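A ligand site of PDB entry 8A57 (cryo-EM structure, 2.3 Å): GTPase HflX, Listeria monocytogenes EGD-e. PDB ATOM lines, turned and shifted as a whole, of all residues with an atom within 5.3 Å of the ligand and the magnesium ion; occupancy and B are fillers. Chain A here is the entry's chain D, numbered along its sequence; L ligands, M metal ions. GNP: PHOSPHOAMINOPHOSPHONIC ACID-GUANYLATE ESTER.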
ATOM      1  N   TYR A 201      23.058 -26.243  26.035  1.00  0.00           N
ATOM      2  CA  TYR A 201      21.882 -25.360  26.249  1.00  0.00           C
ATOM      3  C   TYR A 201      22.386 -23.928  26.450  1.00  0.00           C
ATOM      4  O   TYR A 201      23.549 -23.770  26.870  1.00  0.00           O
ATOM      5  CB  TYR A 201      21.103 -25.805  27.494  1.00  0.00           C
ATOM      6  CG  TYR A 201      19.611 -25.780  27.350  1.00  0.00           C
ATOM      7  CD1 TYR A 201      18.847 -24.733  27.853  1.00  0.00           C
ATOM      8  CD2 TYR A 201      18.952 -26.822  26.719  1.00  0.00           C
ATOM      9  CE1 TYR A 201      17.458 -24.726  27.713  1.00  0.00           C
ATOM     10  CE2 TYR A 201      17.576 -26.832  26.569  1.00  0.00           C
ATOM     11  CZ  TYR A 201      16.833 -25.775  27.068  1.00  0.00           C
ATOM     12  OH  TYR A 201      15.470 -25.814  26.907  1.00  0.00           O
ATOM     13  N   THR A 202      21.542 -22.935  26.183  1.00  0.00           N
ATOM     14  CA  THR A 202      21.854 -21.508  26.448  1.00  0.00           C
ATOM     15  C   THR A 202      22.170 -21.339  27.945  1.00  0.00           C
ATOM     16  O   THR A 202      21.646 -22.128  28.754  1.00  0.00           O
ATOM     17  CB  THR A 202      20.711 -20.607  25.975  1.00  0.00           C
ATOM     18  OG1 THR A 202      19.513 -21.023  26.645  1.00  0.00           O
ATOM     19  CG2 THR A 202      20.508 -20.672  24.482  1.00  0.00           C
ATOM     20  N   ASN A 203      22.996 -20.342  28.289  1.00  0.00           N
ATOM     21  CA  ASN A 203      23.492 -20.047  29.653  1.00  0.00           C
ATOM     22  C   ASN A 203      24.376 -21.179  30.202  1.00  0.00           C
ATOM     23  O   ASN A 203      24.929 -20.997  31.302  1.00  0.00           O
ATOM     24  CB  ASN A 203      22.370 -19.728  30.642  1.00  0.00           C
ATOM     25  CG  ASN A 203      21.899 -18.288  30.581  1.00  0.00           C
ATOM     26  OD1 ASN A 203      22.201 -17.567  29.630  1.00  0.00           O
ATOM     27  ND2 ASN A 203      21.156 -17.870  31.589  1.00  0.00           N
ATOM     28  N   ALA A 204      24.538 -22.293  29.470  1.00  0.00           N
ATOM     29  CA  ALA A 204      25.322 -23.465  29.924  1.00  0.00           C
ATOM     30  C   ALA A 204      26.734 -23.027  30.347  1.00  0.00           C
ATOM     31  O   ALA A 204      27.267 -23.613  31.305  1.00  0.00           O
ATOM     32  CB  ALA A 204      25.369 -24.511  28.839  1.00  0.00           C
ATOM     33  N   GLY A 205      27.316 -22.024  29.678  1.00  0.00           N
ATOM     34  CA  GLY A 205      28.617 -21.431  30.054  1.00  0.00           C
ATOM     35  C   GLY A 205      29.706 -21.706  29.032  1.00  0.00           C
ATOM     36  O   GLY A 205      30.894 -21.550  29.395  1.00  0.00           O
ATOM     37  N   LYS A 206      29.353 -22.045  27.792  1.00  0.00           N
ATOM     38  CA  LYS A 206      30.333 -22.568  26.788  1.00  0.00           C
ATOM     39  C   LYS A 206      31.139 -21.400  26.213  1.00  0.00           C
ATOM     40  O   LYS A 206      32.368 -21.557  26.091  1.00  0.00           O
ATOM     41  CB  LYS A 206      29.629 -23.429  25.733  1.00  0.00           C
ATOM     42  CG  LYS A 206      28.348 -22.880  25.150  1.00  0.00           C
ATOM     43  CD  LYS A 206      27.579 -23.911  24.345  1.00  0.00           C
ATOM     44  CE  LYS A 206      26.458 -23.285  23.543  1.00  0.00           C
ATOM     45  NZ  LYS A 206      25.603 -22.412  24.393  1.00  0.00           N
ATOM     46  N   SER A 207      30.500 -20.265  25.916  1.00  0.00           N
ATOM     47  CA  SER A 207      31.186 -19.011  25.490  1.00  0.00           C
ATOM     48  C   SER A 207      32.119 -18.536  26.608  1.00  0.00           C
ATOM     49  O   SER A 207      33.028 -17.737  26.307  1.00  0.00           O
ATOM     50  CB  SER A 207      30.210 -17.924  25.098  1.00  0.00           C
ATOM     51  OG  SER A 207      29.439 -18.289  23.955  1.00  0.00           O
ATOM     52  N   THR A 208      31.898 -18.983  27.851  1.00  0.00           N
ATOM     53  CA  THR A 208      32.739 -18.652  29.038  1.00  0.00           C
ATOM     54  C   THR A 208      33.931 -19.617  29.118  1.00  0.00           C
ATOM     55  O   THR A 208      35.055 -19.144  29.377  1.00  0.00           O
ATOM     56  CB  THR A 208      31.891 -18.670  30.319  1.00  0.00           C
ATOM     57  OG1 THR A 208      30.707 -17.919  30.042  1.00  0.00           O
ATOM     58  CG2 THR A 208      32.629 -18.110  31.514  1.00  0.00           C
ATOM     59  N   THR A 209      33.678 -20.915  28.950  1.00  0.00           N
ATOM     60  CA  THR A 209      34.717 -21.976  28.820  1.00  0.00           C
ATOM     61  C   THR A 209      35.727 -21.530  27.761  1.00  0.00           C
ATOM     62  O   THR A 209      36.936 -21.553  28.040  1.00  0.00           O
ATOM     63  CB  THR A 209      34.098 -23.329  28.465  1.00  0.00           C
ATOM     64  OG1 THR A 209      33.187 -23.657  29.505  1.00  0.00           O
ATOM     65  CG2 THR A 209      35.125 -24.436  28.303  1.00  0.00           C
ATOM     66  N   VAL A 225      35.256 -13.816  23.615  1.00  0.00           N
ATOM     67  CA  VAL A 225      33.874 -13.868  23.050  1.00  0.00           C
ATOM     68  C   VAL A 225      32.898 -13.222  24.043  1.00  0.00           C
ATOM     69  O   VAL A 225      33.229 -13.140  25.238  1.00  0.00           O
ATOM     70  CB  VAL A 225      33.500 -15.326  22.701  1.00  0.00           C
ATOM     71  CG1 VAL A 225      32.002 -15.551  22.539  1.00  0.00           C
ATOM     72  CG2 VAL A 225      34.251 -15.803  21.467  1.00  0.00           C
ATOM     73  N   PHE A 226      31.749 -12.762  23.543  1.00  0.00           N
ATOM     74  CA  PHE A 226      30.650 -12.141  24.333  1.00  0.00           C
ATOM     75  C   PHE A 226      30.044 -13.176  25.293  1.00  0.00           C
ATOM     76  O   PHE A 226      29.593 -14.244  24.816  1.00  0.00           O
ATOM     77  CB  PHE A 226      29.583 -11.575  23.400  1.00  0.00           C
ATOM     78  CG  PHE A 226      28.404 -10.933  24.099  1.00  0.00           C
ATOM     79  CD1 PHE A 226      27.120 -11.420  23.901  1.00  0.00           C
ATOM     80  CD2 PHE A 226      28.594  -9.857  24.948  1.00  0.00           C
ATOM     81  CE1 PHE A 226      26.037 -10.828  24.545  1.00  0.00           C
ATOM     82  CE2 PHE A 226      27.514  -9.263  25.582  1.00  0.00           C
ATOM     83  CZ  PHE A 226      26.239  -9.750  25.387  1.00  0.00           C
ATOM     84  N   GLU A 227      30.040 -12.867  26.592  1.00  0.00           N
ATOM     85  CA  GLU A 227      29.437 -13.706  27.665  1.00  0.00           C
ATOM     86  C   GLU A 227      28.502 -12.825  28.506  1.00  0.00           C
ATOM     87  O   GLU A 227      28.887 -11.683  28.800  1.00  0.00           O
ATOM     88  CB  GLU A 227      30.525 -14.371  28.516  1.00  0.00           C
ATOM     89  CG  GLU A 227      31.346 -13.404  29.355  1.00  0.00           C
ATOM     90  CD  GLU A 227      32.500 -14.043  30.112  1.00  0.00           C
ATOM     91  OE1 GLU A 227      33.201 -13.319  30.852  1.00  0.00           O
ATOM     92  OE2 GLU A 227      32.708 -15.268  29.960  1.00  0.00           O
ATOM     93  N   LYS A 228      27.324 -13.345  28.853  1.00  0.00           N
ATOM     94  CA  LYS A 228      26.278 -12.596  29.603  1.00  0.00           C
ATOM     95  C   LYS A 228      25.178 -13.571  30.036  1.00  0.00           C
ATOM     96  O   LYS A 228      25.032 -14.624  29.380  1.00  0.00           O
ATOM     97  CB  LYS A 228      25.696 -11.477  28.723  1.00  0.00           C
ATOM     98  CG  LYS A 228      25.000 -10.354  29.484  1.00  0.00           C
ATOM     99  CD  LYS A 228      24.335  -9.344  28.566  1.00  0.00           C
ATOM    100  CE  LYS A 228      23.486  -8.335  29.313  1.00  0.00           C
ATOM    101  NZ  LYS A 228      22.795  -7.414  28.375  1.00  0.00           N
ATOM    102  N   ASP A 229      24.431 -13.230  31.095  1.00  0.00           N
ATOM    103  CA  ASP A 229      23.363 -14.077  31.692  1.00  0.00           C
ATOM    104  C   ASP A 229      22.029 -13.754  30.987  1.00  0.00           C
ATOM    105  O   ASP A 229      21.090 -13.275  31.672  1.00  0.00           O
ATOM    106  CB  ASP A 229      23.292 -13.881  33.206  1.00  0.00           C
ATOM    107  CG  ASP A 229      22.456 -14.922  33.939  1.00  0.00           C
ATOM    108  OD1 ASP A 229      22.323 -14.800  35.176  1.00  0.00           O
ATOM    109  OD2 ASP A 229      21.952 -15.852  33.270  1.00  0.00           O
ATOM    110  N   MET A 230      21.975 -14.002  29.672  1.00  0.00           N
ATOM    111  CA  MET A 230      20.743 -13.882  28.848  1.00  0.00           C
ATOM    112  C   MET A 230      20.621 -15.134  27.969  1.00  0.00           C
ATOM    113  O   MET A 230      21.653 -15.800  27.760  1.00  0.00           O
ATOM    114  CB  MET A 230      20.779 -12.649  27.937  1.00  0.00           C
ATOM    115  CG  MET A 230      22.065 -12.522  27.121  1.00  0.00           C
ATOM    116  SD  MET A 230      22.125 -11.097  26.005  1.00  0.00           S
ATOM    117  CE  MET A 230      20.389 -10.887  25.575  1.00  0.00           C
ATOM    118  N   LEU A 231      19.419 -15.402  27.460  1.00  0.00           N
ATOM    119  CA  LEU A 231      19.142 -16.543  26.547  1.00  0.00           C
ATOM    120  C   LEU A 231      19.583 -16.165  25.132  1.00  0.00           C
ATOM    121  O   LEU A 231      19.216 -15.068  24.659  1.00  0.00           O
ATOM    122  CB  LEU A 231      17.649 -16.860  26.602  1.00  0.00           C
ATOM    123  CG  LEU A 231      17.115 -17.275  27.978  1.00  0.00           C
ATOM    124  CD1 LEU A 231      15.636 -17.623  27.896  1.00  0.00           C
ATOM    125  CD2 LEU A 231      17.893 -18.453  28.534  1.00  0.00           C
ATOM    126  N   PHE A 232      20.373 -17.050  24.493  1.00  0.00           N
ATOM    127  CA  PHE A 232      20.869 -16.915  23.097  1.00  0.00           C
ATOM    128  C   PHE A 232      21.832 -15.719  22.995  1.00  0.00           C
ATOM    129  O   PHE A 232      21.650 -14.896  22.081  1.00  0.00           O
ATOM    130  CB  PHE A 232      19.722 -16.728  22.107  1.00  0.00           C
ATOM    131  CG  PHE A 232      18.635 -17.761  22.170  1.00  0.00           C
ATOM    132  CD1 PHE A 232      18.867 -19.070  21.761  1.00  0.00           C
ATOM    133  CD2 PHE A 232      17.361 -17.432  22.630  1.00  0.00           C
ATOM    134  CE1 PHE A 232      17.856 -20.018  21.814  1.00  0.00           C
ATOM    135  CE2 PHE A 232      16.360 -18.390  22.685  1.00  0.00           C
ATOM    136  CZ  PHE A 232      16.601 -19.679  22.281  1.00  0.00           C
ATOM    137  N   ALA A 233      22.795 -15.617  23.908  1.00  0.00           N
ATOM    138  CA  ALA A 233      23.819 -14.548  23.928  1.00  0.00           C
ATOM    139  C   ALA A 233      24.631 -14.619  22.625  1.00  0.00           C
ATOM    140  O   ALA A 233      24.715 -13.586  21.926  1.00  0.00           O
ATOM    141  CB  ALA A 233      24.703 -14.684  25.140  1.00  0.00           C
ATOM    142  N   THR A 234      25.171 -15.800  22.305  1.00  0.00           N
ATOM    143  CA  THR A 234      25.909 -16.081  21.044  1.00  0.00           C
ATOM    144  C   THR A 234      24.912 -16.535  19.975  1.00  0.00           C
ATOM    145  O   THR A 234      23.999 -17.312  20.331  1.00  0.00           O
ATOM    146  CB  THR A 234      26.977 -17.148  21.243  1.00  0.00           C
ATOM    147  OG1 THR A 234      27.651 -16.920  22.476  1.00  0.00           O
ATOM    148  CG2 THR A 234      27.965 -17.176  20.097  1.00  0.00           C
ATOM    149  N   ASP A 254      33.036 -22.243  19.384  1.00  0.00           N
ATOM    150  CA  ASP A 254      31.863 -21.969  20.248  1.00  0.00           C
ATOM    151  C   ASP A 254      30.674 -21.633  19.343  1.00  0.00           C
ATOM    152  O   ASP A 254      30.808 -20.704  18.526  1.00  0.00           O
ATOM    153  CB  ASP A 254      32.210 -20.858  21.248  1.00  0.00           C
ATOM    154  CG  ASP A 254      31.039 -20.218  21.959  1.00  0.00           C
ATOM    155  OD1 ASP A 254      30.091 -20.957  22.332  1.00  0.00           O
ATOM    156  OD2 ASP A 254      31.071 -18.990  22.143  1.00  0.00           O
ATOM    157  N   THR A 255      29.546 -22.347  19.495  1.00  0.00           N
ATOM    158  CA  THR A 255      28.386 -22.328  18.550  1.00  0.00           C
ATOM    159  C   THR A 255      27.186 -21.605  19.172  1.00  0.00           C
ATOM    160  O   THR A 255      27.295 -21.119  20.318  1.00  0.00           O
ATOM    161  CB  THR A 255      27.970 -23.751  18.164  1.00  0.00           C
ATOM    162  OG1 THR A 255      27.422 -24.398  19.313  1.00  0.00           O
ATOM    163  CG2 THR A 255      29.119 -24.577  17.617  1.00  0.00           C
ATOM    164  N   VAL A 256      26.076 -21.574  18.430  1.00  0.00           N
ATOM    165  CA  VAL A 256      24.722 -21.161  18.924  1.00  0.00           C
ATOM    166  C   VAL A 256      24.333 -22.122  20.045  1.00  0.00           C
ATOM    167  O   VAL A 256      24.797 -23.286  20.021  1.00  0.00           O
ATOM    168  CB  VAL A 256      23.645 -21.187  17.815  1.00  0.00           C
ATOM    169  CG1 VAL A 256      22.364 -20.514  18.273  1.00  0.00           C
ATOM    170  CG2 VAL A 256      24.131 -20.571  16.510  1.00  0.00           C
ATOM    171  N   GLY A 257      23.516 -21.654  20.979  1.00  0.00           N
ATOM    172  CA  GLY A 257      22.911 -22.509  22.019  1.00  0.00           C
ATOM    173  C   GLY A 257      21.678 -23.220  21.497  1.00  0.00           C
ATOM    174  O   GLY A 257      21.186 -22.848  20.413  1.00  0.00           O
ATOM    175  N   ASN A 320      28.955 -28.127  34.256  1.00  0.00           N
ATOM    176  CA  ASN A 320      29.549 -26.791  34.508  1.00  0.00           C
ATOM    177  C   ASN A 320      28.833 -26.134  35.695  1.00  0.00           C
ATOM    178  O   ASN A 320      27.845 -26.710  36.187  1.00  0.00           O
ATOM    179  CB  ASN A 320      29.507 -25.950  33.214  1.00  0.00           C
ATOM    180  CG  ASN A 320      30.127 -24.577  33.364  1.00  0.00           C
ATOM    181  OD1 ASN A 320      31.279 -24.461  33.785  1.00  0.00           O
ATOM    182  ND2 ASN A 320      29.387 -23.540  33.015  1.00  0.00           N
ATOM    183  N   LYS A 321      29.335 -24.969  36.137  1.00  0.00           N
ATOM    184  CA  LYS A 321      28.792 -24.155  37.257  1.00  0.00           C
ATOM    185  C   LYS A 321      28.735 -25.007  38.534  1.00  0.00           C
ATOM    186  O   LYS A 321      27.701 -24.985  39.219  1.00  0.00           O
ATOM    187  CB  LYS A 321      27.417 -23.573  36.916  1.00  0.00           C
ATOM    188  CG  LYS A 321      27.313 -22.849  35.578  1.00  0.00           C
ATOM    189  CD  LYS A 321      26.371 -21.655  35.576  1.00  0.00           C
ATOM    190  CE  LYS A 321      26.054 -21.181  34.177  1.00  0.00           C
ATOM    191  NZ  LYS A 321      25.092 -20.058  34.170  1.00  0.00           N
ATOM    192  N   ALA A 322      29.828 -25.725  38.845  1.00  0.00           N
ATOM    193  CA  ALA A 322      29.985 -26.561  40.054  1.00  0.00           C
ATOM    194  C   ALA A 322      30.019 -25.677  41.303  1.00  0.00           C
ATOM    195  O   ALA A 322      29.499 -26.115  42.345  1.00  0.00           O
ATOM    196  CB  ALA A 322      31.227 -27.406  39.946  1.00  0.00           C
ATOM    197  N   ASP A 323      30.611 -24.482  41.199  1.00  0.00           N
ATOM    198  CA  ASP A 323      30.806 -23.512  42.305  1.00  0.00           C
ATOM    199  C   ASP A 323      29.469 -23.174  42.970  1.00  0.00           C
ATOM    200  O   ASP A 323      29.473 -22.935  44.197  1.00  0.00           O
ATOM    201  CB  ASP A 323      31.506 -22.239  41.823  1.00  0.00           C
ATOM    202  CG  ASP A 323      30.794 -21.521  40.682  1.00  0.00           C
ATOM    203  OD1 ASP A 323      29.796 -22.076  40.172  1.00  0.00           O
ATOM    204  OD2 ASP A 323      31.236 -20.424  40.315  1.00  0.00           O
ATOM    205  N   LEU A 324      28.379 -23.126  42.193  1.00  0.00           N
ATOM    206  CA  LEU A 324      27.005 -22.794  42.680  1.00  0.00           C
ATOM    207  C   LEU A 324      26.546 -23.825  43.710  1.00  0.00           C
ATOM    208  O   LEU A 324      25.680 -23.467  44.552  1.00  0.00           O
ATOM    209  CB  LEU A 324      26.043 -22.724  41.490  1.00  0.00           C
ATOM    210  CG  LEU A 324      26.237 -21.549  40.528  1.00  0.00           C
ATOM    211  CD1 LEU A 324      25.149 -21.532  39.465  1.00  0.00           C
ATOM    212  CD2 LEU A 324      26.265 -20.222  41.289  1.00  0.00           C
ATOM    213  N   PHE A 340      33.241 -29.325  36.628  1.00  0.00           N
ATOM    214  CA  PHE A 340      34.192 -28.177  36.652  1.00  0.00           C
ATOM    215  C   PHE A 340      33.419 -26.861  36.755  1.00  0.00           C
ATOM    216  O   PHE A 340      32.191 -26.860  36.551  1.00  0.00           O
ATOM    217  CB  PHE A 340      35.125 -28.258  35.441  1.00  0.00           C
ATOM    218  CG  PHE A 340      34.627 -27.683  34.146  1.00  0.00           C
ATOM    219  CD1 PHE A 340      33.288 -27.732  33.770  1.00  0.00           C
ATOM    220  CD2 PHE A 340      35.522 -27.113  33.253  1.00  0.00           C
ATOM    221  CE1 PHE A 340      32.858 -27.189  32.571  1.00  0.00           C
ATOM    222  CE2 PHE A 340      35.092 -26.571  32.054  1.00  0.00           C
ATOM    223  CZ  PHE A 340      33.765 -26.614  31.713  1.00  0.00           C
ATOM    224  N   SER A 341      34.122 -25.771  37.060  1.00  0.00           N
ATOM    225  CA  SER A 341      33.585 -24.383  37.131  1.00  0.00           C
ATOM    226  C   SER A 341      34.344 -23.490  36.137  1.00  0.00           C
ATOM    227  O   SER A 341      35.553 -23.259  36.340  1.00  0.00           O
ATOM    228  CB  SER A 341      33.671 -23.833  38.531  1.00  0.00           C
ATOM    229  OG  SER A 341      33.268 -22.465  38.560  1.00  0.00           O
ATOM    230  N   ALA A 342      33.632 -23.010  35.106  1.00  0.00           N
ATOM    231  CA  ALA A 342      34.180 -22.234  33.966  1.00  0.00           C
ATOM    232  C   ALA A 342      34.874 -20.960  34.465  1.00  0.00           C
ATOM    233  O   ALA A 342      35.802 -20.487  33.764  1.00  0.00           O
ATOM    234  CB  ALA A 342      33.060 -21.917  32.992  1.00  0.00           C
ATOM    235  N   ARG A 343      34.439 -20.419  35.603  1.00  0.00           N
ATOM    236  CA  ARG A 343      35.023 -19.220  36.249  1.00  0.00           C
ATOM    237  C   ARG A 343      36.483 -19.502  36.627  1.00  0.00           C
ATOM    238  O   ARG A 343      37.321 -18.586  36.482  1.00  0.00           O
ATOM    239  CB  ARG A 343      34.253 -18.829  37.518  1.00  0.00           C
ATOM    240  CG  ARG A 343      32.769 -18.552  37.310  1.00  0.00           C
ATOM    241  CD  ARG A 343      32.495 -17.275  36.524  1.00  0.00           C
ATOM    242  NE  ARG A 343      31.117 -16.844  36.670  1.00  0.00           N
ATOM    243  CZ  ARG A 343      30.554 -15.845  35.996  1.00  0.00           C
ATOM    244  NH1 ARG A 343      31.214 -15.259  35.013  1.00  0.00           N
ATOM    245  NH2 ARG A 343      29.339 -15.432  36.307  1.00  0.00           N
HETATM  246  PG  GNP L   1      24.587 -18.928  24.687  1.00  0.00           P
HETATM  247  O1G GNP L   1      25.818 -18.499  23.934  1.00  0.00           O
HETATM  248  O2G GNP L   1      23.717 -19.778  23.800  1.00  0.00           O
HETATM  249  O3G GNP L   1      23.826 -17.713  25.143  1.00  0.00           O
HETATM  250  N3B GNP L   1      25.034 -19.816  25.974  1.00  0.00           N
HETATM  251  PB  GNP L   1      26.522 -19.750  26.611  1.00  0.00           P
HETATM  252  O1B GNP L   1      26.896 -21.014  27.331  1.00  0.00           O
HETATM  253  O2B GNP L   1      27.450 -19.216  25.554  1.00  0.00           O
HETATM  254  O3A GNP L   1      26.448 -18.608  27.725  1.00  0.00           O
HETATM  255  PA  GNP L   1      27.608 -18.062  28.683  1.00  0.00           P
HETATM  256  O1A GNP L   1      28.850 -18.855  28.415  1.00  0.00           O
HETATM  257  O2A GNP L   1      27.670 -16.577  28.558  1.00  0.00           O
HETATM  258  O5' GNP L   1      27.034 -18.470  30.132  1.00  0.00           O
HETATM  259  C5' GNP L   1      26.018 -17.642  30.766  1.00  0.00           C
HETATM  260  C4' GNP L   1      26.624 -16.888  31.915  1.00  0.00           C
HETATM  261  O4' GNP L   1      26.715 -17.767  33.059  1.00  0.00           O
HETATM  262  C3' GNP L   1      28.053 -16.381  31.715  1.00  0.00           C
HETATM  263  O3' GNP L   1      28.035 -15.124  31.055  1.00  0.00           O
HETATM  264  C2' GNP L   1      28.571 -16.277  33.150  1.00  0.00           C
HETATM  265  O2' GNP L   1      28.278 -15.038  33.752  1.00  0.00           O
HETATM  266  C1' GNP L   1      27.825 -17.411  33.850  1.00  0.00           C
HETATM  267  N9  GNP L   1      28.644 -18.607  34.048  1.00  0.00           N
HETATM  268  C8  GNP L   1      29.202 -19.400  33.071  1.00  0.00           C
HETATM  269  N7  GNP L   1      29.865 -20.419  33.559  1.00  0.00           N
HETATM  270  C5  GNP L   1      29.747 -20.287  34.937  1.00  0.00           C
HETATM  271  C6  GNP L   1      30.257 -21.097  35.981  1.00  0.00           C
HETATM  272  O6  GNP L   1      30.955 -22.114  35.893  1.00  0.00           O
HETATM  273  N1  GNP L   1      29.894 -20.601  37.235  1.00  0.00           N
HETATM  274  C2  GNP L   1      29.121 -19.484  37.454  1.00  0.00           C
HETATM  275  N2  GNP L   1      28.874 -19.159  38.734  1.00  0.00           N
HETATM  276  N3  GNP L   1      28.646 -18.722  36.475  1.00  0.00           N
HETATM  277  C4  GNP L   1      28.990 -19.183  35.252  1.00  0.00           C
HETATM  278 MG    MG M   1      27.580 -17.662  24.330  1.00  0.00          MG
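O of Phe 226 touches the magnesium ion, at 3.996 Å. Three residues have an atom within 4 Å of the magnesium ion: Ser 207, Phe 226 and Thr 234.
O of Gly 205 sits at hydrogen-bond distance from OG1 of Thr 209, 3.1 Å away. OE2 of Glu 227 sits close to OG1 of Thr 208 (3.3 Å). The backbone NH of Ala 342 lies within hydrogen-bond range of the side-chain amide oxygen of Asn 320 (3.1 Å). The backbone carbonyl oxygen (O) of Asn 203 sits at hydrogen-bond distance from the side-chain amino group (NZ) of Lys 321 (3.0 Å). The backbone carbonyl oxygen of Phe 340 is in hydrogen-bond range of the backbone NH of Lys 321 (3.5 Å). OD2 of Asp 323 lies within hydrogen-bond range of OG of Ser 341 (3.4 Å). The side-chain amide oxygen of Asn 203 sits close to the backbone carbonyl oxygen of Met 230. The backbone carbonyl oxygen (O) of Ala 204 lies within hydrogen-bond range of the side-chain amide nitrogen (ND2) of Asn 320, at 2.7 Å.
The backbone NH of Ser 207 sits at hydrogen-bond distance from an oxygen (O1A) of the ligand, at 3.3 Å. The backbone NH of Thr 234 sits close to an oxygen (O1G) of the ligand, at 3.2 Å. An oxygen (O1B) of the ligand sits at hydrogen-bond distance from the backbone NH (N) of Gly 205, 2.6 Å away. The backbone NH (N) of Thr 208 sits at hydrogen-bond distance from an oxygen (O1A) of the ligand. OG1 of Thr 208 lies within hydrogen-bond range of O1A of the ligand, at 2.6 Å. The backbone NH of Ala 233 is in hydrogen-bond range of an oxygen (O3G) of the ligand. N of Lys 206 sits at hydrogen-bond distance from O1B of the ligand, at 2.7 Å. The side-chain amino group (NZ) of Lys 206 lies within salt-bridge range of an oxygen (O2G) of the ligand. The guanidinium group of Arg 343 is in hydrogen-bond range of an oxygen (O2') of the ligand, 2.8 Å away. The backbone NH of Lys 228 sits at hydrogen-bond distance from an oxygen (O3') of the ligand (2.9 Å). An oxygen (O3') of the ligand lies close to the backbone carbonyl oxygen (O) of Lys 228, at 3.5 Å. The backbone NH (N) of Ala 342 lies within hydrogen-bond range of an oxygen (O6) of the ligand, at 2.9 Å. O6 of the ligand sits close to N of Lys 321, 3.3 Å away. O4' of the ligand sits at hydrogen-bond distance from NZ of Lys 321 (3.0 Å). OD2 of Asp 323 lies within hydrogen-bond range of N2 of the ligand (3.1 Å). O6 of the ligand sits close to OD1 of Asn 320 (3.2 Å). O2G of the ligand sits close to N of Gly 257 (3.4 Å). O1B of the ligand lies within hydrogen-bond range of N of Ala 204 (3.4 Å).
N3B of the ligand sits close to N of Asn 203 (3.1 Å). Merely in contact with the ligand: Thr 202 (3.4 Å), Glu 227 (3.5 Å), Met 230 (3.9 Å), Phe 232 (3.5 Å), Leu 324 (3.8 Å) and Ser 341 (3.5 Å).
The magnesium ion is bound by O2B of the ligand (2.0 Å), O1G of the ligand (2.0 Å), OG of Ser 207 (2.0 Å) and OG1 of Thr 234 (2.0 Å). The magnesium ion has four donor atoms within binding distance.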
